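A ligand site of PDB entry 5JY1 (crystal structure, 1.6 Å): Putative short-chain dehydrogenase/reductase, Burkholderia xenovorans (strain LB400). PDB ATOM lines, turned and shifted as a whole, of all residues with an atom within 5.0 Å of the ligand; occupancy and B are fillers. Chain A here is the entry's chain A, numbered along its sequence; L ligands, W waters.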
ATOM      1  N   GLY A  21       8.465  12.528  -4.573  1.00  0.00           N
ATOM      2  CA  GLY A  21       8.395  13.845  -5.178  1.00  0.00           C
ATOM      3  C   GLY A  21       9.481  14.105  -6.199  1.00  0.00           C
ATOM      4  O   GLY A  21       9.897  15.257  -6.360  1.00  0.00           O
ATOM      5  N   ALA A  22       9.936  13.076  -6.906  1.00  0.00           N
ATOM      6  CA  ALA A  22      11.080  13.186  -7.794  1.00  0.00           C
ATOM      7  C   ALA A  22      10.739  13.718  -9.182  1.00  0.00           C
ATOM      8  O   ALA A  22      11.597  13.680 -10.067  1.00  0.00           O
ATOM      9  CB  ALA A  22      11.762  11.820  -7.931  1.00  0.00           C
ATOM     10  N   GLY A  23       9.507  14.211  -9.386  1.00  0.00           N
ATOM     11  CA  GLY A  23       9.171  14.802 -10.679  1.00  0.00           C
ATOM     12  C   GLY A  23       9.728  16.195 -10.895  1.00  0.00           C
ATOM     13  O   GLY A  23       9.852  16.618 -12.041  1.00  0.00           O
ATOM     14  N   GLY A  24      10.066  16.914  -9.825  1.00  0.00           N
ATOM     15  CA  GLY A  24      10.546  18.262  -9.972  1.00  0.00           C
ATOM     16  C   GLY A  24      11.502  18.661  -8.868  1.00  0.00           C
ATOM     17  O   GLY A  24      11.764  17.894  -7.935  1.00  0.00           O
ATOM     18  N   GLY A  25      12.043  19.871  -9.006  1.00  0.00           N
ATOM     19  CA  GLY A  25      12.783  20.507  -7.914  1.00  0.00           C
ATOM     20  C   GLY A  25      13.971  19.699  -7.448  1.00  0.00           C
ATOM     21  O   GLY A  25      14.730  19.130  -8.229  1.00  0.00           O
ATOM     22  N   ILE A  26      14.129  19.658  -6.117  1.00  0.00           N
ATOM     23  CA  ILE A  26      15.281  18.961  -5.545  1.00  0.00           C
ATOM     24  C   ILE A  26      15.174  17.458  -5.762  1.00  0.00           C
ATOM     25  O   ILE A  26      16.177  16.789  -6.051  1.00  0.00           O
ATOM     26  CB  ILE A  26      15.423  19.319  -4.047  1.00  0.00           C
ATOM     27  CG1 ILE A  26      15.915  20.762  -3.922  1.00  0.00           C
ATOM     28  CG2 ILE A  26      16.374  18.364  -3.377  1.00  0.00           C
ATOM     29  CD1 ILE A  26      16.034  21.277  -2.482  1.00  0.00           C
ATOM     30  N   GLY A  27      13.968  16.903  -5.652  1.00  0.00           N
ATOM     31  CA  GLY A  27      13.803  15.470  -5.840  1.00  0.00           C
ATOM     32  C   GLY A  27      14.238  15.024  -7.222  1.00  0.00           C
ATOM     33  O   GLY A  27      14.857  13.964  -7.377  1.00  0.00           O
ATOM     34  N   ALA A  44       8.948   8.139  -7.313  1.00  0.00           N
ATOM     35  CA  ALA A  44       7.706   7.970  -6.559  1.00  0.00           C
ATOM     36  C   ALA A  44       7.013   9.324  -6.461  1.00  0.00           C
ATOM     37  O   ALA A  44       7.156  10.053  -5.484  1.00  0.00           O
ATOM     38  CB  ALA A  44       7.998   7.362  -5.190  1.00  0.00           C
ATOM     39  N   GLU A  45       6.215   9.635  -7.488  1.00  0.00           N
ATOM     40  CA  GLU A  45       5.722  10.979  -7.748  1.00  0.00           C
ATOM     41  C   GLU A  45       4.222  10.941  -8.030  1.00  0.00           C
ATOM     42  O   GLU A  45       3.737  10.013  -8.682  1.00  0.00           O
ATOM     43  CB  GLU A  45       6.510  11.585  -8.941  1.00  0.00           C
ATOM     44  CG  GLU A  45       5.952  12.863  -9.530  1.00  0.00           C
ATOM     45  CD  GLU A  45       5.937  14.003  -8.546  1.00  0.00           C
ATOM     46  OE1 GLU A  45       7.000  14.328  -7.968  1.00  0.00           O
ATOM     47  OE2 GLU A  45       4.837  14.580  -8.339  1.00  0.00           O
ATOM     48  N   ILE A  46       3.485  11.940  -7.538  1.00  0.00           N
ATOM     49  CA  ILE A  46       2.038  11.966  -7.742  1.00  0.00           C
ATOM     50  C   ILE A  46       1.658  12.556  -9.111  1.00  0.00           C
ATOM     51  O   ILE A  46       0.630  12.173  -9.694  1.00  0.00           O
ATOM     52  CB  ILE A  46       1.338  12.728  -6.597  1.00  0.00           C
ATOM     53  CG1 ILE A  46      -0.173  12.450  -6.581  1.00  0.00           C
ATOM     54  CG2 ILE A  46       1.623  14.228  -6.685  1.00  0.00           C
ATOM     55  CD1 ILE A  46      -0.854  12.890  -5.290  1.00  0.00           C
ATOM     56  N   ASN A  47       2.477  13.456  -9.636  1.00  0.00           N
ATOM     57  CA  ASN A  47       2.235  14.086 -10.934  1.00  0.00           C
ATOM     58  C   ASN A  47       2.745  13.140 -12.015  1.00  0.00           C
ATOM     59  O   ASN A  47       3.956  12.974 -12.176  1.00  0.00           O
ATOM     60  CB  ASN A  47       2.927  15.441 -11.006  1.00  0.00           C
ATOM     61  CG  ASN A  47       2.616  16.204 -12.294  1.00  0.00           C
ATOM     62  OD1 ASN A  47       2.393  15.613 -13.351  1.00  0.00           O
ATOM     63  ND2 ASN A  47       2.625  17.527 -12.209  1.00  0.00           N
ATOM     64  N   THR A  50       5.199  14.911 -14.893  1.00  0.00           N
ATOM     65  CA  THR A  50       6.591  15.192 -14.531  1.00  0.00           C
ATOM     66  C   THR A  50       7.305  13.930 -14.063  1.00  0.00           C
ATOM     67  O   THR A  50       8.516  13.797 -14.276  1.00  0.00           O
ATOM     68  CB  THR A  50       6.651  16.275 -13.461  1.00  0.00           C
ATOM     69  OG1 THR A  50       5.979  15.825 -12.277  1.00  0.00           O
ATOM     70  CG2 THR A  50       5.978  17.549 -13.963  1.00  0.00           C
ATOM     71  N   THR A  70       2.689   7.565  -6.998  1.00  0.00           N
ATOM     72  CA  THR A  70       2.712   7.450  -5.548  1.00  0.00           C
ATOM     73  C   THR A  70       2.130   8.704  -4.933  1.00  0.00           C
ATOM     74  O   THR A  70       2.507   9.814  -5.308  1.00  0.00           O
ATOM     75  CB  THR A  70       4.147   7.242  -5.026  1.00  0.00           C
ATOM     76  OG1 THR A  70       4.743   6.115  -5.675  1.00  0.00           O
ATOM     77  CG2 THR A  70       4.161   7.012  -3.525  1.00  0.00           C
ATOM     78  N   ASP A  71       1.209   8.524  -3.981  1.00  0.00           N
ATOM     79  CA  ASP A  71       0.624   9.612  -3.190  1.00  0.00           C
ATOM     80  C   ASP A  71       1.089   9.386  -1.759  1.00  0.00           C
ATOM     81  O   ASP A  71       0.588   8.493  -1.075  1.00  0.00           O
ATOM     82  CB  ASP A  71      -0.907   9.593  -3.298  1.00  0.00           C
ATOM     83  CG  ASP A  71      -1.571  10.738  -2.527  1.00  0.00           C
ATOM     84  OD1 ASP A  71      -0.921  11.373  -1.677  1.00  0.00           O
ATOM     85  OD2 ASP A  71      -2.778  10.977  -2.766  1.00  0.00           O
ATOM     86  N   VAL A  72       2.048  10.201  -1.300  1.00  0.00           N
ATOM     87  CA  VAL A  72       2.662   9.979   0.008  1.00  0.00           C
ATOM     88  C   VAL A  72       1.734  10.361   1.157  1.00  0.00           C
ATOM     89  O   VAL A  72       2.102  10.185   2.323  1.00  0.00           O
ATOM     90  CB  VAL A  72       4.000  10.733   0.148  1.00  0.00           C
ATOM     91  CG1 VAL A  72       4.996  10.276  -0.939  1.00  0.00           C
ATOM     92  CG2 VAL A  72       3.797  12.240   0.105  1.00  0.00           C
ATOM     93  N   THR A  73       0.540  10.870   0.853  1.00  0.00           N
ATOM     94  CA  THR A  73      -0.471  11.015   1.895  1.00  0.00           C
ATOM     95  C   THR A  73      -1.200   9.703   2.176  1.00  0.00           C
ATOM     96  O   THR A  73      -2.025   9.661   3.100  1.00  0.00           O
ATOM     97  CB  THR A  73      -1.493  12.106   1.541  1.00  0.00           C
ATOM     98  OG1 THR A  73      -2.266  11.706   0.410  1.00  0.00           O
ATOM     99  CG2 THR A  73      -0.781  13.418   1.227  1.00  0.00           C
ATOM    100  N   ASN A  97      13.192  10.958   1.258  1.00  0.00           N
ATOM    101  CA  ASN A  97      11.861  11.467   1.583  1.00  0.00           C
ATOM    102  C   ASN A  97      11.851  12.960   1.290  1.00  0.00           C
ATOM    103  O   ASN A  97      12.238  13.780   2.116  1.00  0.00           O
ATOM    104  CB  ASN A  97      11.498  11.151   3.026  1.00  0.00           C
ATOM    105  CG  ASN A  97      11.313   9.664   3.255  1.00  0.00           C
ATOM    106  OD1 ASN A  97      10.531   9.008   2.562  1.00  0.00           O
ATOM    107  ND2 ASN A  97      12.051   9.104   4.204  1.00  0.00           N
ATOM    108  N   ASN A  98      11.381  13.315   0.096  1.00  0.00           N
ATOM    109  CA  ASN A  98      11.561  14.655  -0.432  1.00  0.00           C
ATOM    110  C   ASN A  98      10.263  15.384  -0.743  1.00  0.00           C
ATOM    111  O   ASN A  98      10.269  16.620  -0.745  1.00  0.00           O
ATOM    112  CB  ASN A  98      12.443  14.567  -1.697  1.00  0.00           C
ATOM    113  CG  ASN A  98      12.389  15.801  -2.553  1.00  0.00           C
ATOM    114  OD1 ASN A  98      13.177  16.730  -2.385  1.00  0.00           O
ATOM    115  ND2 ASN A  98      11.463  15.808  -3.507  1.00  0.00           N
ATOM    116  N   ALA A  99       9.145  14.670  -0.937  1.00  0.00           N
ATOM    117  CA  ALA A  99       7.914  15.281  -1.397  1.00  0.00           C
ATOM    118  C   ALA A  99       7.450  16.411  -0.467  1.00  0.00           C
ATOM    119  O   ALA A  99       7.620  16.345   0.750  1.00  0.00           O
ATOM    120  CB  ALA A  99       6.816  14.221  -1.517  1.00  0.00           C
ATOM    121  N   PHE A 100       6.809  17.418  -1.060  1.00  0.00           N
ATOM    122  CA  PHE A 100       6.418  18.626  -0.338  1.00  0.00           C
ATOM    123  C   PHE A 100       5.156  19.208  -0.959  1.00  0.00           C
ATOM    124  O   PHE A 100       5.005  19.209  -2.185  1.00  0.00           O
ATOM    125  CB  PHE A 100       7.570  19.639  -0.364  1.00  0.00           C
ATOM    126  CG  PHE A 100       7.158  21.051  -0.109  1.00  0.00           C
ATOM    127  CD1 PHE A 100       6.918  21.490   1.183  1.00  0.00           C
ATOM    128  CD2 PHE A 100       7.020  21.949  -1.150  1.00  0.00           C
ATOM    129  CE1 PHE A 100       6.540  22.792   1.434  1.00  0.00           C
ATOM    130  CE2 PHE A 100       6.648  23.257  -0.905  1.00  0.00           C
ATOM    131  CZ  PHE A 100       6.408  23.679   0.387  1.00  0.00           C
ATOM    132  N   VAL A 101       4.253  19.691  -0.111  1.00  0.00           N
ATOM    133  CA  VAL A 101       3.061  20.436  -0.541  1.00  0.00           C
ATOM    134  C   VAL A 101       2.967  21.707   0.291  1.00  0.00           C
ATOM    135  O   VAL A 101       2.951  21.637   1.527  1.00  0.00           O
ATOM    136  CB  VAL A 101       1.776  19.598  -0.389  1.00  0.00           C
ATOM    137  CG1 VAL A 101       0.579  20.441  -0.763  1.00  0.00           C
ATOM    138  CG2 VAL A 101       1.836  18.366  -1.267  1.00  0.00           C
ATOM    139  N   PHE A 149      14.616  15.138   4.501  1.00  0.00           N
ATOM    140  CA  PHE A 149      14.815  16.556   4.217  1.00  0.00           C
ATOM    141  C   PHE A 149      14.066  17.398   5.239  1.00  0.00           C
ATOM    142  O   PHE A 149      12.861  17.218   5.427  1.00  0.00           O
ATOM    143  CB  PHE A 149      14.368  16.915   2.797  1.00  0.00           C
ATOM    144  CG  PHE A 149      15.374  16.568   1.740  1.00  0.00           C
ATOM    145  CD1 PHE A 149      16.374  17.457   1.414  1.00  0.00           C
ATOM    146  CD2 PHE A 149      15.339  15.344   1.101  1.00  0.00           C
ATOM    147  CE1 PHE A 149      17.326  17.140   0.453  1.00  0.00           C
ATOM    148  CE2 PHE A 149      16.282  15.027   0.130  1.00  0.00           C
ATOM    149  CZ  PHE A 149      17.266  15.928  -0.199  1.00  0.00           C
ATOM    150  N   TYR A 150      14.781  18.296   5.899  1.00  0.00           N
ATOM    151  CA  TYR A 150      14.108  19.258   6.771  1.00  0.00           C
ATOM    152  C   TYR A 150      14.447  20.638   6.231  1.00  0.00           C
ATOM    153  O   TYR A 150      14.668  20.772   5.017  1.00  0.00           O
ATOM    154  CB  TYR A 150      14.477  19.021   8.251  1.00  0.00           C
ATOM    155  CG  TYR A 150      15.828  19.529   8.724  1.00  0.00           C
ATOM    156  CD1 TYR A 150      17.012  18.939   8.298  1.00  0.00           C
ATOM    157  CD2 TYR A 150      15.909  20.559   9.661  1.00  0.00           C
ATOM    158  CE1 TYR A 150      18.246  19.401   8.749  1.00  0.00           C
ATOM    159  CE2 TYR A 150      17.116  21.021  10.120  1.00  0.00           C
ATOM    160  CZ  TYR A 150      18.278  20.442   9.666  1.00  0.00           C
ATOM    161  OH  TYR A 150      19.479  20.916  10.131  1.00  0.00           O
ATOM    162  N   SER A 151      14.478  21.667   7.068  1.00  0.00           N
ATOM    163  CA  SER A 151      14.658  23.008   6.540  1.00  0.00           C
ATOM    164  C   SER A 151      15.319  23.898   7.580  1.00  0.00           C
ATOM    165  O   SER A 151      15.088  23.764   8.784  1.00  0.00           O
ATOM    166  CB  SER A 151      13.329  23.631   6.098  1.00  0.00           C
ATOM    167  OG  SER A 151      13.522  24.978   5.689  1.00  0.00           O
ATOM    168  N   TYR A 164       4.846  24.238   8.673  1.00  0.00           N
ATOM    169  CA  TYR A 164       6.009  23.617   8.044  1.00  0.00           C
ATOM    170  C   TYR A 164       7.147  23.449   9.046  1.00  0.00           C
ATOM    171  O   TYR A 164       7.749  22.368   9.141  1.00  0.00           O
ATOM    172  CB  TYR A 164       6.406  24.489   6.868  1.00  0.00           C
ATOM    173  CG  TYR A 164       7.624  24.098   6.090  1.00  0.00           C
ATOM    174  CD1 TYR A 164       7.557  23.137   5.098  1.00  0.00           C
ATOM    175  CD2 TYR A 164       8.847  24.726   6.319  1.00  0.00           C
ATOM    176  CE1 TYR A 164       8.672  22.782   4.375  1.00  0.00           C
ATOM    177  CE2 TYR A 164       9.963  24.387   5.596  1.00  0.00           C
ATOM    178  CZ  TYR A 164       9.870  23.415   4.619  1.00  0.00           C
ATOM    179  OH  TYR A 164      10.976  23.060   3.887  1.00  0.00           O
ATOM    180  N   LYS A 168       8.638  19.780   9.986  1.00  0.00           N
ATOM    181  CA  LYS A 168      10.019  19.467   9.629  1.00  0.00           C
ATOM    182  C   LYS A 168      10.911  19.319  10.853  1.00  0.00           C
ATOM    183  O   LYS A 168      11.885  18.548  10.827  1.00  0.00           O
ATOM    184  CB  LYS A 168      10.570  20.543   8.678  1.00  0.00           C
ATOM    185  CG  LYS A 168       9.929  20.574   7.277  1.00  0.00           C
ATOM    186  CD  LYS A 168      10.196  19.285   6.510  1.00  0.00           C
ATOM    187  CE  LYS A 168      10.018  19.498   5.006  1.00  0.00           C
ATOM    188  NZ  LYS A 168      10.442  18.295   4.219  1.00  0.00           N
ATOM    189  N   PRO A 194      18.351  21.620   2.755  1.00  0.00           N
ATOM    190  CA  PRO A 194      18.864  22.191   1.501  1.00  0.00           C
ATOM    191  C   PRO A 194      18.250  23.547   1.203  1.00  0.00           C
ATOM    192  O   PRO A 194      17.178  23.889   1.718  1.00  0.00           O
ATOM    193  CB  PRO A 194      18.417  21.162   0.465  1.00  0.00           C
ATOM    194  CG  PRO A 194      17.013  20.777   0.991  1.00  0.00           C
ATOM    195  CD  PRO A 194      17.128  20.819   2.528  1.00  0.00           C
ATOM    196  N   THR A 195      18.920  24.341   0.365  1.00  0.00           N
ATOM    197  CA  THR A 195      18.238  25.399  -0.370  1.00  0.00           C
ATOM    198  C   THR A 195      18.622  25.253  -1.832  1.00  0.00           C
ATOM    199  O   THR A 195      19.774  24.935  -2.145  1.00  0.00           O
ATOM    200  CB  THR A 195      18.561  26.817   0.143  1.00  0.00           C
ATOM    201  OG1 THR A 195      19.941  27.128  -0.104  1.00  0.00           O
ATOM    202  CG2 THR A 195      18.285  26.911   1.626  1.00  0.00           C
ATOM    203  N   ALA A 196      17.658  25.473  -2.718  1.00  0.00           N
ATOM    204  CA  ALA A 196      17.949  25.333  -4.146  1.00  0.00           C
ATOM    205  C   ALA A 196      16.831  25.976  -4.957  1.00  0.00           C
ATOM    206  O   ALA A 196      15.762  26.324  -4.434  1.00  0.00           O
ATOM    207  CB  ALA A 196      18.134  23.869  -4.552  1.00  0.00           C
ATOM    208  N   GLY A 198      14.097  25.542  -6.726  1.00  0.00           N
ATOM    209  CA  GLY A 198      12.972  24.671  -6.993  1.00  0.00           C
ATOM    210  C   GLY A 198      11.717  25.446  -7.337  1.00  0.00           C
ATOM    211  O   GLY A 198      11.777  26.614  -7.741  1.00  0.00           O
ATOM    212  N   ALA A 199      10.560  24.787  -7.177  1.00  0.00           N
ATOM    213  CA  ALA A 199       9.304  25.405  -7.571  1.00  0.00           C
ATOM    214  C   ALA A 199       9.036  26.682  -6.782  1.00  0.00           C
ATOM    215  O   ALA A 199       8.588  27.689  -7.341  1.00  0.00           O
ATOM    216  CB  ALA A 199       8.141  24.411  -7.402  1.00  0.00           C
ATOM    217  N   THR A 200       9.313  26.658  -5.473  1.00  0.00           N
ATOM    218  CA  THR A 200       9.099  27.849  -4.648  1.00  0.00           C
ATOM    219  C   THR A 200      10.009  28.992  -5.086  1.00  0.00           C
ATOM    220  O   THR A 200       9.590  30.159  -5.107  1.00  0.00           O
ATOM    221  CB  THR A 200       9.339  27.520  -3.178  1.00  0.00           C
ATOM    222  OG1 THR A 200       8.422  26.498  -2.764  1.00  0.00           O
ATOM    223  CG2 THR A 200       9.141  28.752  -2.298  1.00  0.00           C
HETATM  224  P1  LIG L   1       9.006  21.194  -5.107  1.00  0.00           P
HETATM  225  O1  LIG L   1       7.733  21.911  -4.762  1.00  0.00           O
HETATM  226  O2  LIG L   1       9.793  21.858  -6.227  1.00  0.00           O
HETATM  227  O3  LIG L   1       8.699  19.610  -5.512  1.00  0.00           O
HETATM  228  C1  LIG L   1       7.800  18.926  -4.703  1.00  0.00           C
HETATM  229  C2  LIG L   1       7.510  17.518  -5.361  1.00  0.00           C
HETATM  230  O4  LIG L   1       6.778  16.834  -4.562  1.00  0.00           O
HETATM  231  C3  LIG L   1       6.649  17.753  -6.659  1.00  0.00           C
HETATM  232  O5  LIG L   1       7.175  17.009  -7.716  1.00  0.00           O
HETATM  233  C4  LIG L   1       5.286  17.263  -6.245  1.00  0.00           C
HETATM  234  O6  LIG L   1       4.464  16.875  -7.447  1.00  0.00           O
HETATM  235  C5  LIG L   1       5.583  16.247  -5.469  1.00  0.00           C
HETATM  236  N1  LIG L   1       4.468  15.894  -4.601  1.00  0.00           N
HETATM  237  C6  LIG L   1       3.632  16.756  -4.017  1.00  0.00           C
HETATM  238  N2  LIG L   1       2.753  16.060  -3.320  1.00  0.00           N
HETATM  239  C7  LIG L   1       3.050  14.770  -3.467  1.00  0.00           C
HETATM  240  C8  LIG L   1       2.432  13.622  -2.955  1.00  0.00           C
HETATM  241  N3  LIG L   1       1.299  13.349  -2.078  1.00  0.00           N
HETATM  242  N4  LIG L   1       2.915  12.428  -3.253  1.00  0.00           N
HETATM  243  C9  LIG L   1       4.012  12.326  -4.070  1.00  0.00           C
HETATM  244  N5  LIG L   1       4.616  13.423  -4.578  1.00  0.00           N
HETATM  245  C10 LIG L   1       4.111  14.662  -4.256  1.00  0.00           C
HETATM  246  O7  LIG L   1       9.917  21.105  -3.740  1.00  0.00           O
HETATM  247  P2  LIG L   1      11.505  21.477  -3.541  1.00  0.00           P
HETATM  248  O8  LIG L   1      11.648  22.990  -3.483  1.00  0.00           O
HETATM  249  O9  LIG L   1      12.417  20.917  -4.641  1.00  0.00           O
HETATM  250  O10 LIG L   1      11.926  20.882  -2.052  1.00  0.00           O
HETATM  251  C11 LIG L   1      12.113  19.474  -1.912  1.00  0.00           C
HETATM  252  C12 LIG L   1      12.427  19.133  -0.416  1.00  0.00           C
HETATM  253  O11 LIG L   1      13.361  19.955   0.059  1.00  0.00           O
HETATM  254  C13 LIG L   1      11.176  19.381   0.427  1.00  0.00           C
HETATM  255  O12 LIG L   1      11.073  18.483   1.423  1.00  0.00           O
HETATM  256  C14 LIG L   1      11.421  20.800   1.001  1.00  0.00           C
HETATM  257  O13 LIG L   1      10.557  20.956   2.197  1.00  0.00           O
HETATM  258  C15 LIG L   1      12.717  20.798   1.268  1.00  0.00           C
HETATM  259  N6  LIG L   1      13.289  22.130   1.261  1.00  0.00           N
HETATM  260  C16 LIG L   1      13.570  22.760   0.093  1.00  0.00           C
HETATM  261  C17 LIG L   1      14.125  24.052   0.082  1.00  0.00           C
HETATM  262  C18 LIG L   1      14.431  24.762  -1.203  1.00  0.00           C
HETATM  263  O14 LIG L   1      15.076  25.799  -1.204  1.00  0.00           O
HETATM  264  N7  LIG L   1      13.961  24.256  -2.432  1.00  0.00           N
HETATM  265  C19 LIG L   1      14.394  24.667   1.274  1.00  0.00           C
HETATM  266  C20 LIG L   1      14.129  24.043   2.446  1.00  0.00           C
HETATM  267  C21 LIG L   1      13.577  22.751   2.443  1.00  0.00           C
HETATM  268  O   HOH W   1      11.427  18.081  -5.119  1.00  0.00           O
HETATM  269  O   HOH W   2      12.032  26.364   3.815  1.00  0.00           O
HETATM  270  O   HOH W   3       3.438  18.951  -9.459  1.00  0.00           O
HETATM  271  O   HOH W   4       9.164  21.277  -8.968  1.00  0.00           O
HETATM  272  O   HOH W   5       6.320  17.734 -10.394  1.00  0.00           O
HETATM  273  O   HOH W   6      12.790  27.910  -2.351  1.00  0.00           O
HETATM  274  O   HOH W   7      -0.137  17.220  -4.326  1.00  0.00           O
HETATM  275  O   HOH W   8       9.433  24.334  -3.694  1.00  0.00           O
HETATM  276  O   HOH W   9      12.273  26.158  -4.135  1.00  0.00           O
HETATM  277  O   HOH W  10      -0.618  15.691  -1.647  1.00  0.00           O
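The backbone carbonyl oxygen (O) of Asn 98 sits at hydrogen-bond distance from an oxygen (O12) of the ligand, 3.0 Å away. The side-chain hydroxyl of Tyr 164 lies within hydrogen-bond range of an oxygen (O13) of the ligand, 2.7 Å away. N of Ala 196 lies within hydrogen-bond range of O14 of the ligand. The backbone NH (N) of Val 72 sits at hydrogen-bond distance from a nitrogen (N4) of the ligand (3.1 Å). N3 of the ligand sits at hydrogen-bond distance from OD1 of Asp 71, 3.0 Å away. The side-chain amino group (NZ) of Lys 168 lies within hydrogen-bond range of an oxygen (O12) of the ligand, 2.9 Å away. N of Ile 46 is in hydrogen-bond range of N5 of the ligand (3.5 Å). The backbone carbonyl oxygen (O) of Ala 196 lies within hydrogen-bond range of a nitrogen (N7) of the ligand (3.4 Å). The backbone NH (N) of Ala 199 sits at hydrogen-bond distance from an oxygen (O2) of the ligand (3.2 Å). OE2 of Glu 45 sits at hydrogen-bond distance from O6 of the ligand (2.5 Å). N of Ile 26 is in hydrogen-bond range of O9 of the ligand (2.6 Å).
The side-chain hydroxyl of Thr 73 sits at hydrogen-bond distance from the side-chain carboxylate of Asp 71 (2.5 Å). The side-chain amide oxygen of Asn 98 sits at hydrogen-bond distance from the backbone NH of Gly 27 (3.4 Å). The backbone NH of Gly 23 is in hydrogen-bond range of the side-chain carboxylate of Glu 45 (2.9 Å). The side-chain amide nitrogen (ND2) of Asn 98 sits at hydrogen-bond distance from the backbone carbonyl oxygen (O) of Gly 21 (3.3 Å). O of Ala 44 lies within hydrogen-bond range of N of Gly 21 (2.9 Å). OE2 of Glu 45 is in hydrogen-bond range of N of Asn 47. O of Thr 70 lies within hydrogen-bond range of N of Ile 46. O of Glu 45 is in hydrogen-bond range of N of Thr 70, at 3.2 Å.
Water W8 lies within hydrogen-bond range of the side-chain hydroxyl (OG1) of Thr 200 and an oxygen (O8) of the ligand. Water W4 bridges O2 of the ligand (2.9 Å) and N of Gly 25 (3.2 Å). Water W5 lies within hydrogen-bond range of OG1 of Thr 50 (2.7 Å) and O5 of the ligand (2.9 Å). Water W3 bridges an oxygen (O6) of the ligand and the side-chain amide nitrogen of Asn 47. Water W2 bridges OG of Ser 151 and OH of Tyr 164.
A nitrogen (N4) of the ligand sits close to the backbone carbonyl oxygen (O) of Thr 70 (3.3 Å). Residues that only touch the ligand: Gly 21 (3.4 Å), Gly 24 (3.6 Å), Gly 25 (3.3 Å), Thr 73 (3.9 Å), Ala 99 (3.7 Å), Phe 100 (3.4 Å), Val 101 (3.2 Å), Phe 149 (3.9 Å), Tyr 150 (3.4 Å), Ser 151 (3.4 Å), Pro 194 (2.9 Å) and Thr 195 (3.3 Å). Hydrophobic or aromatic side chains within 4 Å of the ligand: Ile 26, Ile 46, Val 72, Ala 99, Phe 100, Val 101, Phe 149, Tyr 164, Pro 194 and Ala 199. Of the 32 residues printed, 23 come within 4 Å of the ligand. The nearest printed residue that does not touch the ligand is Gly 23 (4.01 Å).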
